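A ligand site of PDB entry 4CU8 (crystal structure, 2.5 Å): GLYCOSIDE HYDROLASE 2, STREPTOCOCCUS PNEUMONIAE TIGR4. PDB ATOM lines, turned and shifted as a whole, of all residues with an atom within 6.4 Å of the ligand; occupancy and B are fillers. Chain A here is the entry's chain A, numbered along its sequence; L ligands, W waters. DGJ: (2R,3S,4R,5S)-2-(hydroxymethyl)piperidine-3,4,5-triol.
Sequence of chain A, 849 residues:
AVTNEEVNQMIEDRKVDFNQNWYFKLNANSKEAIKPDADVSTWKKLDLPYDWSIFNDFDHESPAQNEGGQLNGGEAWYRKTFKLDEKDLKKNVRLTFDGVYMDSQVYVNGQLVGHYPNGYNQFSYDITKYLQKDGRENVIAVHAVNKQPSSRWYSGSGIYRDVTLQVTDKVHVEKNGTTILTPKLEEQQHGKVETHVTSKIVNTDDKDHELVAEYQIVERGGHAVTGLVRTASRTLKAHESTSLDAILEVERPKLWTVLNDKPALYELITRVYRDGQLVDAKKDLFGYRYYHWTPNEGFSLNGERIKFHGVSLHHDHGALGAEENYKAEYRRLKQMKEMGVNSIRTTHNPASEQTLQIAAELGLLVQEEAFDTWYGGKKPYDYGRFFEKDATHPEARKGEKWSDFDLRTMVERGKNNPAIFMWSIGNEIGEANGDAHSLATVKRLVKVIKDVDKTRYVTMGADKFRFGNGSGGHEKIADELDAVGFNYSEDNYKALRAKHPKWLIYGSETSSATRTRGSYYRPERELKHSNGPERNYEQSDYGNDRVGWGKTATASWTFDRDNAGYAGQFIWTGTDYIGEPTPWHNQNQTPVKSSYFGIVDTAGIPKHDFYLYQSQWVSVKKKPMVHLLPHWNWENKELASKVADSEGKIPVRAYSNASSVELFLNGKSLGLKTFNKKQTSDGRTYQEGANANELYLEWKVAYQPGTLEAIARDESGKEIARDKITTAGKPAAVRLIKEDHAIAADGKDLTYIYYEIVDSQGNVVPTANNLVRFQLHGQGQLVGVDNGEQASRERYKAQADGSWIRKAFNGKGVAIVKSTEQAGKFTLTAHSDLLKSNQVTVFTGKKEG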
ATOM      1  N   ARG A 152      21.548   6.443  28.323  1.00  0.00           N
ATOM      2  CA  ARG A 152      21.870   6.051  26.918  1.00  0.00           C
ATOM      3  C   ARG A 152      21.013   6.821  25.908  1.00  0.00           C
ATOM      4  O   ARG A 152      21.103   6.535  24.702  1.00  0.00           O
ATOM      5  CB  ARG A 152      21.683   4.551  26.711  1.00  0.00           C
ATOM      6  CG  ARG A 152      22.462   3.670  27.682  1.00  0.00           C
ATOM      7  CD  ARG A 152      22.392   2.180  27.288  1.00  0.00           C
ATOM      8  NE  ARG A 152      21.021   1.676  27.364  1.00  0.00           N
ATOM      9  CZ  ARG A 152      20.201   1.562  26.317  1.00  0.00           C
ATOM     10  NH1 ARG A 152      20.612   1.911  25.105  1.00  0.00           N
ATOM     11  NH2 ARG A 152      18.966   1.067  26.488  1.00  0.00           N
ATOM     12  N   TRP A 153      20.189   7.751  26.377  1.00  0.00           N
ATOM     13  CA  TRP A 153      19.313   8.564  25.507  1.00  0.00           C
ATOM     14  C   TRP A 153      19.120   9.922  26.133  1.00  0.00           C
ATOM     15  O   TRP A 153      19.555  10.156  27.259  1.00  0.00           O
ATOM     16  CB  TRP A 153      17.932   7.918  25.282  1.00  0.00           C
ATOM     17  CG  TRP A 153      17.188   7.630  26.567  1.00  0.00           C
ATOM     18  CD1 TRP A 153      16.329   8.475  27.235  1.00  0.00           C
ATOM     19  CD2 TRP A 153      17.237   6.409  27.352  1.00  0.00           C
ATOM     20  NE1 TRP A 153      15.829   7.868  28.381  1.00  0.00           N
ATOM     21  CE2 TRP A 153      16.365   6.613  28.490  1.00  0.00           C
ATOM     22  CE3 TRP A 153      17.888   5.181  27.206  1.00  0.00           C
ATOM     23  CZ2 TRP A 153      16.147   5.609  29.456  1.00  0.00           C
ATOM     24  CZ3 TRP A 153      17.661   4.183  28.181  1.00  0.00           C
ATOM     25  CH2 TRP A 153      16.802   4.415  29.289  1.00  0.00           C
ATOM     26  N   HIS A 314      10.554   6.517  23.554  1.00  0.00           N
ATOM     27  CA  HIS A 314      11.180   7.263  24.624  1.00  0.00           C
ATOM     28  C   HIS A 314      10.237   8.371  25.034  1.00  0.00           C
ATOM     29  O   HIS A 314       9.160   8.541  24.444  1.00  0.00           O
ATOM     30  CB  HIS A 314      12.573   7.787  24.226  1.00  0.00           C
ATOM     31  CG  HIS A 314      13.675   6.790  24.473  1.00  0.00           C
ATOM     32  ND1 HIS A 314      13.912   6.228  25.715  1.00  0.00           N
ATOM     33  CD2 HIS A 314      14.599   6.237  23.640  1.00  0.00           C
ATOM     34  CE1 HIS A 314      14.921   5.371  25.638  1.00  0.00           C
ATOM     35  NE2 HIS A 314      15.362   5.364  24.395  1.00  0.00           N
ATOM     36  N   ARG A 345       5.592   0.096  24.061  1.00  0.00           N
ATOM     37  CA  ARG A 345       6.537  -0.336  25.077  1.00  0.00           C
ATOM     38  C   ARG A 345       7.168   0.946  25.602  1.00  0.00           C
ATOM     39  O   ARG A 345       7.647   1.742  24.827  1.00  0.00           O
ATOM     40  CB  ARG A 345       7.591  -1.237  24.431  1.00  0.00           C
ATOM     41  CG  ARG A 345       8.579  -1.851  25.412  1.00  0.00           C
ATOM     42  CD  ARG A 345       9.495  -2.872  24.740  1.00  0.00           C
ATOM     43  NE  ARG A 345      10.542  -3.268  25.662  1.00  0.00           N
ATOM     44  CZ  ARG A 345      11.845  -3.346  25.387  1.00  0.00           C
ATOM     45  NH1 ARG A 345      12.324  -3.081  24.148  1.00  0.00           N
ATOM     46  NH2 ARG A 345      12.679  -3.691  26.351  1.00  0.00           N
ATOM     47  N   THR A 347      10.006   2.251  26.709  1.00  0.00           N
ATOM     48  CA  THR A 347      11.428   1.938  26.743  1.00  0.00           C
ATOM     49  C   THR A 347      12.221   3.131  27.327  1.00  0.00           C
ATOM     50  O   THR A 347      12.190   4.207  26.748  1.00  0.00           O
ATOM     51  CB  THR A 347      11.904   1.646  25.317  1.00  0.00           C
ATOM     52  OG1 THR A 347      11.433   2.685  24.448  1.00  0.00           O
ATOM     53  CG2 THR A 347      11.340   0.329  24.841  1.00  0.00           C
ATOM     54  N   HIS A 348      12.905   2.973  28.465  1.00  0.00           N
ATOM     55  CA  HIS A 348      12.991   1.736  29.232  1.00  0.00           C
ATOM     56  C   HIS A 348      12.838   2.167  30.674  1.00  0.00           C
ATOM     57  O   HIS A 348      13.794   2.085  31.473  1.00  0.00           O
ATOM     58  CB  HIS A 348      14.367   1.071  29.040  1.00  0.00           C
ATOM     59  CG  HIS A 348      14.703   0.796  27.597  1.00  0.00           C
ATOM     60  ND1 HIS A 348      14.169  -0.248  26.901  1.00  0.00           N
ATOM     61  CD2 HIS A 348      15.520   1.442  26.720  1.00  0.00           C
ATOM     62  CE1 HIS A 348      14.640  -0.258  25.656  1.00  0.00           C
ATOM     63  NE2 HIS A 348      15.467   0.777  25.530  1.00  0.00           N
ATOM     64  N   ASP A 372      16.355  -0.258  32.908  1.00  0.00           N
ATOM     65  CA  ASP A 372      17.295  -0.418  31.818  1.00  0.00           C
ATOM     66  C   ASP A 372      18.571  -1.158  32.275  1.00  0.00           C
ATOM     67  O   ASP A 372      19.444  -1.512  31.466  1.00  0.00           O
ATOM     68  CB  ASP A 372      17.623   0.923  31.197  1.00  0.00           C
ATOM     69  CG  ASP A 372      18.447   0.777  29.899  1.00  0.00           C
ATOM     70  OD1 ASP A 372      18.080  -0.030  28.988  1.00  0.00           O
ATOM     71  OD2 ASP A 372      19.494   1.501  29.809  1.00  0.00           O
ATOM     72  N   LYS A 378      24.841   0.456  33.213  1.00  0.00           N
ATOM     73  CA  LYS A 378      25.256   0.595  31.800  1.00  0.00           C
ATOM     74  C   LYS A 378      26.068   1.898  31.605  1.00  0.00           C
ATOM     75  O   LYS A 378      26.996   1.943  30.815  1.00  0.00           O
ATOM     76  CB  LYS A 378      24.031   0.582  30.893  1.00  0.00           C
ATOM     77  CG  LYS A 378      23.513  -0.796  30.555  1.00  0.00           C
ATOM     78  CD  LYS A 378      22.256  -0.701  29.738  1.00  0.00           C
ATOM     79  CE  LYS A 378      21.680  -2.094  29.535  1.00  0.00           C
ATOM     80  NZ  LYS A 378      20.273  -1.996  29.053  1.00  0.00           N
ATOM     81  N   ASN A 427      15.350  -4.358  30.342  1.00  0.00           N
ATOM     82  CA  ASN A 427      15.791  -4.326  28.933  1.00  0.00           C
ATOM     83  C   ASN A 427      17.307  -4.568  28.757  1.00  0.00           C
ATOM     84  O   ASN A 427      18.127  -3.837  29.352  1.00  0.00           O
ATOM     85  CB  ASN A 427      15.441  -2.985  28.299  1.00  0.00           C
ATOM     86  CG  ASN A 427      15.986  -2.859  26.890  1.00  0.00           C
ATOM     87  OD1 ASN A 427      15.542  -3.574  25.979  1.00  0.00           O
ATOM     88  ND2 ASN A 427      16.972  -1.970  26.694  1.00  0.00           N
ATOM     89  N   GLU A 428      17.646  -5.546  27.915  1.00  0.00           N
ATOM     90  CA  GLU A 428      19.051  -5.907  27.625  1.00  0.00           C
ATOM     91  C   GLU A 428      19.948  -5.789  28.862  1.00  0.00           C
ATOM     92  O   GLU A 428      20.924  -5.027  28.876  1.00  0.00           O
ATOM     93  CB  GLU A 428      19.622  -5.074  26.473  1.00  0.00           C
ATOM     94  CG  GLU A 428      18.762  -5.139  25.234  1.00  0.00           C
ATOM     95  CD  GLU A 428      19.430  -4.609  23.998  1.00  0.00           C
ATOM     96  OE1 GLU A 428      20.402  -3.835  24.123  1.00  0.00           O
ATOM     97  OE2 GLU A 428      18.959  -4.962  22.902  1.00  0.00           O
ATOM     98  N   ASN A 487      14.859  -9.217  21.728  1.00  0.00           N
ATOM     99  CA  ASN A 487      15.478  -8.087  21.036  1.00  0.00           C
ATOM    100  C   ASN A 487      16.304  -8.532  19.829  1.00  0.00           C
ATOM    101  O   ASN A 487      17.306  -9.207  19.984  1.00  0.00           O
ATOM    102  CB  ASN A 487      16.359  -7.292  21.987  1.00  0.00           C
ATOM    103  CG  ASN A 487      15.564  -6.436  22.984  1.00  0.00           C
ATOM    104  OD1 ASN A 487      16.113  -5.448  23.500  1.00  0.00           O
ATOM    105  ND2 ASN A 487      14.289  -6.802  23.258  1.00  0.00           N
ATOM    106  N   TYR A 488      15.890  -8.159  18.632  1.00  0.00           N
ATOM    107  CA  TYR A 488      16.673  -8.390  17.379  1.00  0.00           C
ATOM    108  C   TYR A 488      17.103  -9.821  17.172  1.00  0.00           C
ATOM    109  O   TYR A 488      18.181 -10.067  16.627  1.00  0.00           O
ATOM    110  CB  TYR A 488      17.895  -7.439  17.305  1.00  0.00           C
ATOM    111  CG  TYR A 488      17.520  -6.002  17.608  1.00  0.00           C
ATOM    112  CD1 TYR A 488      16.922  -5.197  16.627  1.00  0.00           C
ATOM    113  CD2 TYR A 488      17.656  -5.490  18.894  1.00  0.00           C
ATOM    114  CE1 TYR A 488      16.527  -3.903  16.925  1.00  0.00           C
ATOM    115  CE2 TYR A 488      17.262  -4.198  19.207  1.00  0.00           C
ATOM    116  CZ  TYR A 488      16.702  -3.407  18.229  1.00  0.00           C
ATOM    117  OH  TYR A 488      16.329  -2.105  18.544  1.00  0.00           O
ATOM    118  N   GLU A 509      11.948  -5.914  20.899  1.00  0.00           N
ATOM    119  CA  GLU A 509      12.584  -4.808  20.209  1.00  0.00           C
ATOM    120  C   GLU A 509      13.100  -5.262  18.855  1.00  0.00           C
ATOM    121  O   GLU A 509      13.916  -6.199  18.768  1.00  0.00           O
ATOM    122  CB  GLU A 509      13.725  -4.223  21.045  1.00  0.00           C
ATOM    123  CG  GLU A 509      13.737  -2.696  21.056  1.00  0.00           C
ATOM    124  CD  GLU A 509      14.971  -2.119  21.708  1.00  0.00           C
ATOM    125  OE1 GLU A 509      15.040  -2.078  22.951  1.00  0.00           O
ATOM    126  OE2 GLU A 509      15.911  -1.718  20.956  1.00  0.00           O
ATOM    127  N   SER A 512      15.353  -1.295  14.213  1.00  0.00           N
ATOM    128  CA  SER A 512      16.407  -0.289  14.326  1.00  0.00           C
ATOM    129  C   SER A 512      16.921   0.112  12.951  1.00  0.00           C
ATOM    130  O   SER A 512      18.111   0.355  12.787  1.00  0.00           O
ATOM    131  CB  SER A 512      17.575  -0.748  15.190  1.00  0.00           C
ATOM    132  OG  SER A 512      17.422  -0.367  16.533  1.00  0.00           O
ATOM    133  N   VAL A 547      21.068  -0.567  11.167  1.00  0.00           N
ATOM    134  CA  VAL A 547      22.256  -0.788  11.941  1.00  0.00           C
ATOM    135  C   VAL A 547      22.755  -2.244  11.800  1.00  0.00           C
ATOM    136  O   VAL A 547      22.036  -3.134  11.256  1.00  0.00           O
ATOM    137  CB  VAL A 547      22.025  -0.423  13.433  1.00  0.00           C
ATOM    138  CG1 VAL A 547      21.704   1.070  13.589  1.00  0.00           C
ATOM    139  CG2 VAL A 547      20.934  -1.297  14.047  1.00  0.00           C
ATOM    140  N   TRP A 549      23.155  -4.724  13.819  1.00  0.00           N
ATOM    141  CA  TRP A 549      22.327  -5.749  14.470  1.00  0.00           C
ATOM    142  C   TRP A 549      20.863  -5.653  14.103  1.00  0.00           C
ATOM    143  O   TRP A 549      20.057  -6.417  14.626  1.00  0.00           O
ATOM    144  CB  TRP A 549      22.441  -5.589  15.965  1.00  0.00           C
ATOM    145  CG  TRP A 549      22.084  -4.218  16.448  1.00  0.00           C
ATOM    146  CD1 TRP A 549      20.845  -3.786  16.863  1.00  0.00           C
ATOM    147  CD2 TRP A 549      22.965  -3.085  16.598  1.00  0.00           C
ATOM    148  NE1 TRP A 549      20.901  -2.474  17.274  1.00  0.00           N
ATOM    149  CE2 TRP A 549      22.183  -2.014  17.130  1.00  0.00           C
ATOM    150  CE3 TRP A 549      24.340  -2.874  16.361  1.00  0.00           C
ATOM    151  CZ2 TRP A 549      22.725  -0.733  17.394  1.00  0.00           C
ATOM    152  CZ3 TRP A 549      24.882  -1.593  16.625  1.00  0.00           C
ATOM    153  CH2 TRP A 549      24.076  -0.543  17.137  1.00  0.00           C
ATOM    154  N   TRP A 572      11.747  -0.429  17.163  1.00  0.00           N
ATOM    155  CA  TRP A 572      12.631   0.644  17.633  1.00  0.00           C
ATOM    156  C   TRP A 572      12.837   1.619  16.449  1.00  0.00           C
ATOM    157  O   TRP A 572      13.553   1.257  15.523  1.00  0.00           O
ATOM    158  CB  TRP A 572      13.978   0.050  18.110  1.00  0.00           C
ATOM    159  CG  TRP A 572      14.733   1.073  18.852  1.00  0.00           C
ATOM    160  CD1 TRP A 572      15.677   1.951  18.348  1.00  0.00           C
ATOM    161  CD2 TRP A 572      14.585   1.404  20.249  1.00  0.00           C
ATOM    162  NE1 TRP A 572      16.103   2.803  19.341  1.00  0.00           N
ATOM    163  CE2 TRP A 572      15.465   2.503  20.514  1.00  0.00           C
ATOM    164  CE3 TRP A 572      13.794   0.907  21.290  1.00  0.00           C
ATOM    165  CZ2 TRP A 572      15.561   3.103  21.762  1.00  0.00           C
ATOM    166  CZ3 TRP A 572      13.897   1.487  22.526  1.00  0.00           C
ATOM    167  CH2 TRP A 572      14.775   2.579  22.761  1.00  0.00           C
ATOM    168  N   TYR A 577      13.838  10.421  18.873  1.00  0.00           N
ATOM    169  CA  TYR A 577      14.040  10.966  20.202  1.00  0.00           C
ATOM    170  C   TYR A 577      15.411  11.667  20.194  1.00  0.00           C
ATOM    171  O   TYR A 577      16.270  11.381  19.320  1.00  0.00           O
ATOM    172  CB  TYR A 577      13.954   9.865  21.284  1.00  0.00           C
ATOM    173  CG  TYR A 577      14.869   8.673  21.000  1.00  0.00           C
ATOM    174  CD1 TYR A 577      14.475   7.671  20.096  1.00  0.00           C
ATOM    175  CD2 TYR A 577      16.137   8.554  21.630  1.00  0.00           C
ATOM    176  CE1 TYR A 577      15.286   6.595  19.824  1.00  0.00           C
ATOM    177  CE2 TYR A 577      16.966   7.463  21.377  1.00  0.00           C
ATOM    178  CZ  TYR A 577      16.537   6.497  20.466  1.00  0.00           C
ATOM    179  OH  TYR A 577      17.344   5.405  20.170  1.00  0.00           O
ATOM    180  N   GLU A 580      20.979   9.251  21.228  1.00  0.00           N
ATOM    181  CA  GLU A 580      21.370   8.045  20.449  1.00  0.00           C
ATOM    182  C   GLU A 580      21.352   8.153  18.907  1.00  0.00           C
ATOM    183  O   GLU A 580      20.514   7.526  18.249  1.00  0.00           O
ATOM    184  CB  GLU A 580      20.542   6.846  20.937  1.00  0.00           C
ATOM    185  CG  GLU A 580      21.152   5.523  20.558  1.00  0.00           C
ATOM    186  CD  GLU A 580      20.473   4.335  21.222  1.00  0.00           C
ATOM    187  OE1 GLU A 580      19.359   4.544  21.759  1.00  0.00           O
ATOM    188  OE2 GLU A 580      21.084   3.209  21.230  1.00  0.00           O
ATOM    189  N   THR A 582      22.871   6.855  16.369  1.00  0.00           N
ATOM    190  CA  THR A 582      23.417   5.751  15.592  1.00  0.00           C
ATOM    191  C   THR A 582      22.923   5.893  14.145  1.00  0.00           C
ATOM    192  O   THR A 582      21.762   6.171  13.936  1.00  0.00           O
ATOM    193  CB  THR A 582      22.981   4.423  16.230  1.00  0.00           C
ATOM    194  OG1 THR A 582      23.187   4.536  17.649  1.00  0.00           O
ATOM    195  CG2 THR A 582      23.794   3.216  15.696  1.00  0.00           C
ATOM    196  N   PHE A 597      16.115   6.380  14.265  1.00  0.00           N
ATOM    197  CA  PHE A 597      15.359   5.141  14.367  1.00  0.00           C
ATOM    198  C   PHE A 597      13.850   5.305  14.176  1.00  0.00           C
ATOM    199  O   PHE A 597      13.129   4.348  13.862  1.00  0.00           O
ATOM    200  CB  PHE A 597      15.594   4.534  15.743  1.00  0.00           C
ATOM    201  CG  PHE A 597      17.023   4.065  16.002  1.00  0.00           C
ATOM    202  CD1 PHE A 597      17.603   3.054  15.245  1.00  0.00           C
ATOM    203  CD2 PHE A 597      17.746   4.563  17.072  1.00  0.00           C
ATOM    204  CE1 PHE A 597      18.870   2.586  15.512  1.00  0.00           C
ATOM    205  CE2 PHE A 597      19.003   4.093  17.353  1.00  0.00           C
ATOM    206  CZ  PHE A 597      19.576   3.111  16.567  1.00  0.00           C
HETATM  207  C1  DGJ L   1      18.703  -1.748  22.068  1.00  0.00           C
HETATM  208  C2  DGJ L   1      18.371  -0.873  23.257  1.00  0.00           C
HETATM  209  O2  DGJ L   1      17.519  -1.602  24.071  1.00  0.00           O
HETATM  210  C3  DGJ L   1      17.661   0.449  22.808  1.00  0.00           C
HETATM  211  O3  DGJ L   1      17.475   1.367  23.941  1.00  0.00           O
HETATM  212  C4  DGJ L   1      18.517   1.121  21.757  1.00  0.00           C
HETATM  213  O4  DGJ L   1      19.835   1.375  22.327  1.00  0.00           O
HETATM  214  C5  DGJ L   1      18.648   0.173  20.602  1.00  0.00           C
HETATM  215  N5  DGJ L   1      19.437  -1.009  21.025  1.00  0.00           N
HETATM  216  C6  DGJ L   1      19.257   0.853  19.386  1.00  0.00           C
HETATM  217  O6  DGJ L   1      19.278  -0.107  18.323  1.00  0.00           O
HETATM  218  O   HOH W   1      17.711   3.973  24.026  1.00  0.00           O
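Residues that only touch the ligand: Trp 572 (3.2 Å), Glu 428 (3.3 Å), Tyr 488 (3.6 Å) and Phe 597 (3.6 Å).
Within 4 Å of the ligand: Arg 152, His 348, Asn 427, Glu 428, Tyr 488, Glu 509, Ser 512, Trp 549, Trp 572, Glu 580 and Phe 597.
An oxygen (O3) of the ligand sits at hydrogen-bond distance from a ring nitrogen (NE2) of His 348 (2.6 Å).
The side-chain carboxylate (OE2) of Glu 580 sits at hydrogen-bond distance from an oxygen (O4) of the ligand (2.5 Å).
NE1 of Trp 549 is in hydrogen-bond range of O6 of the ligand.
N5 of the ligand lies within salt-bridge range of OE2 of Glu 509 (3.6 Å).
OG of Ser 512 is in hydrogen-bond range of O6 of the ligand.
ND2 of Asn 427 lies within hydrogen-bond range of O2 of the ligand, 2.7 Å away.
NH1 of Arg 152 lies within hydrogen-bond range of O4 of the ligand (2.9 Å).
Water W1 lies within hydrogen-bond range of O3 of the ligand (2.6 Å), NE2 of His 314 (2.8 Å) and OE1 of Glu 580 (2.9 Å).
The side-chain hydroxyl (OH) of Tyr 488 sits at hydrogen-bond distance from the side-chain carboxylate (OE2) of Glu 509 (2.5 Å).
The backbone carbonyl oxygen of Asn 427 lies within hydrogen-bond range of the side-chain amino group of Lys 378 (2.8 Å).
NZ of Lys 378 sits close to O of Glu 428, 3.1 Å away.
OE2 of Glu 428 lies close to OD1 of Asn 487 (2.9 Å).
The side-chain amide oxygen of Asn 427 sits close to the side-chain amide oxygen of Asn 487 (3.2 Å).
N of Ser 512 sits at hydrogen-bond distance from O of Trp 572, 3.4 Å away.
O of Ser 512 lies within hydrogen-bond range of N of Val 547, 3.5 Å away.
The side-chain carboxylate (OE1) of Glu 509 is in salt-bridge range of the guanidinium group (NH1) of Arg 345 (3.1 Å).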
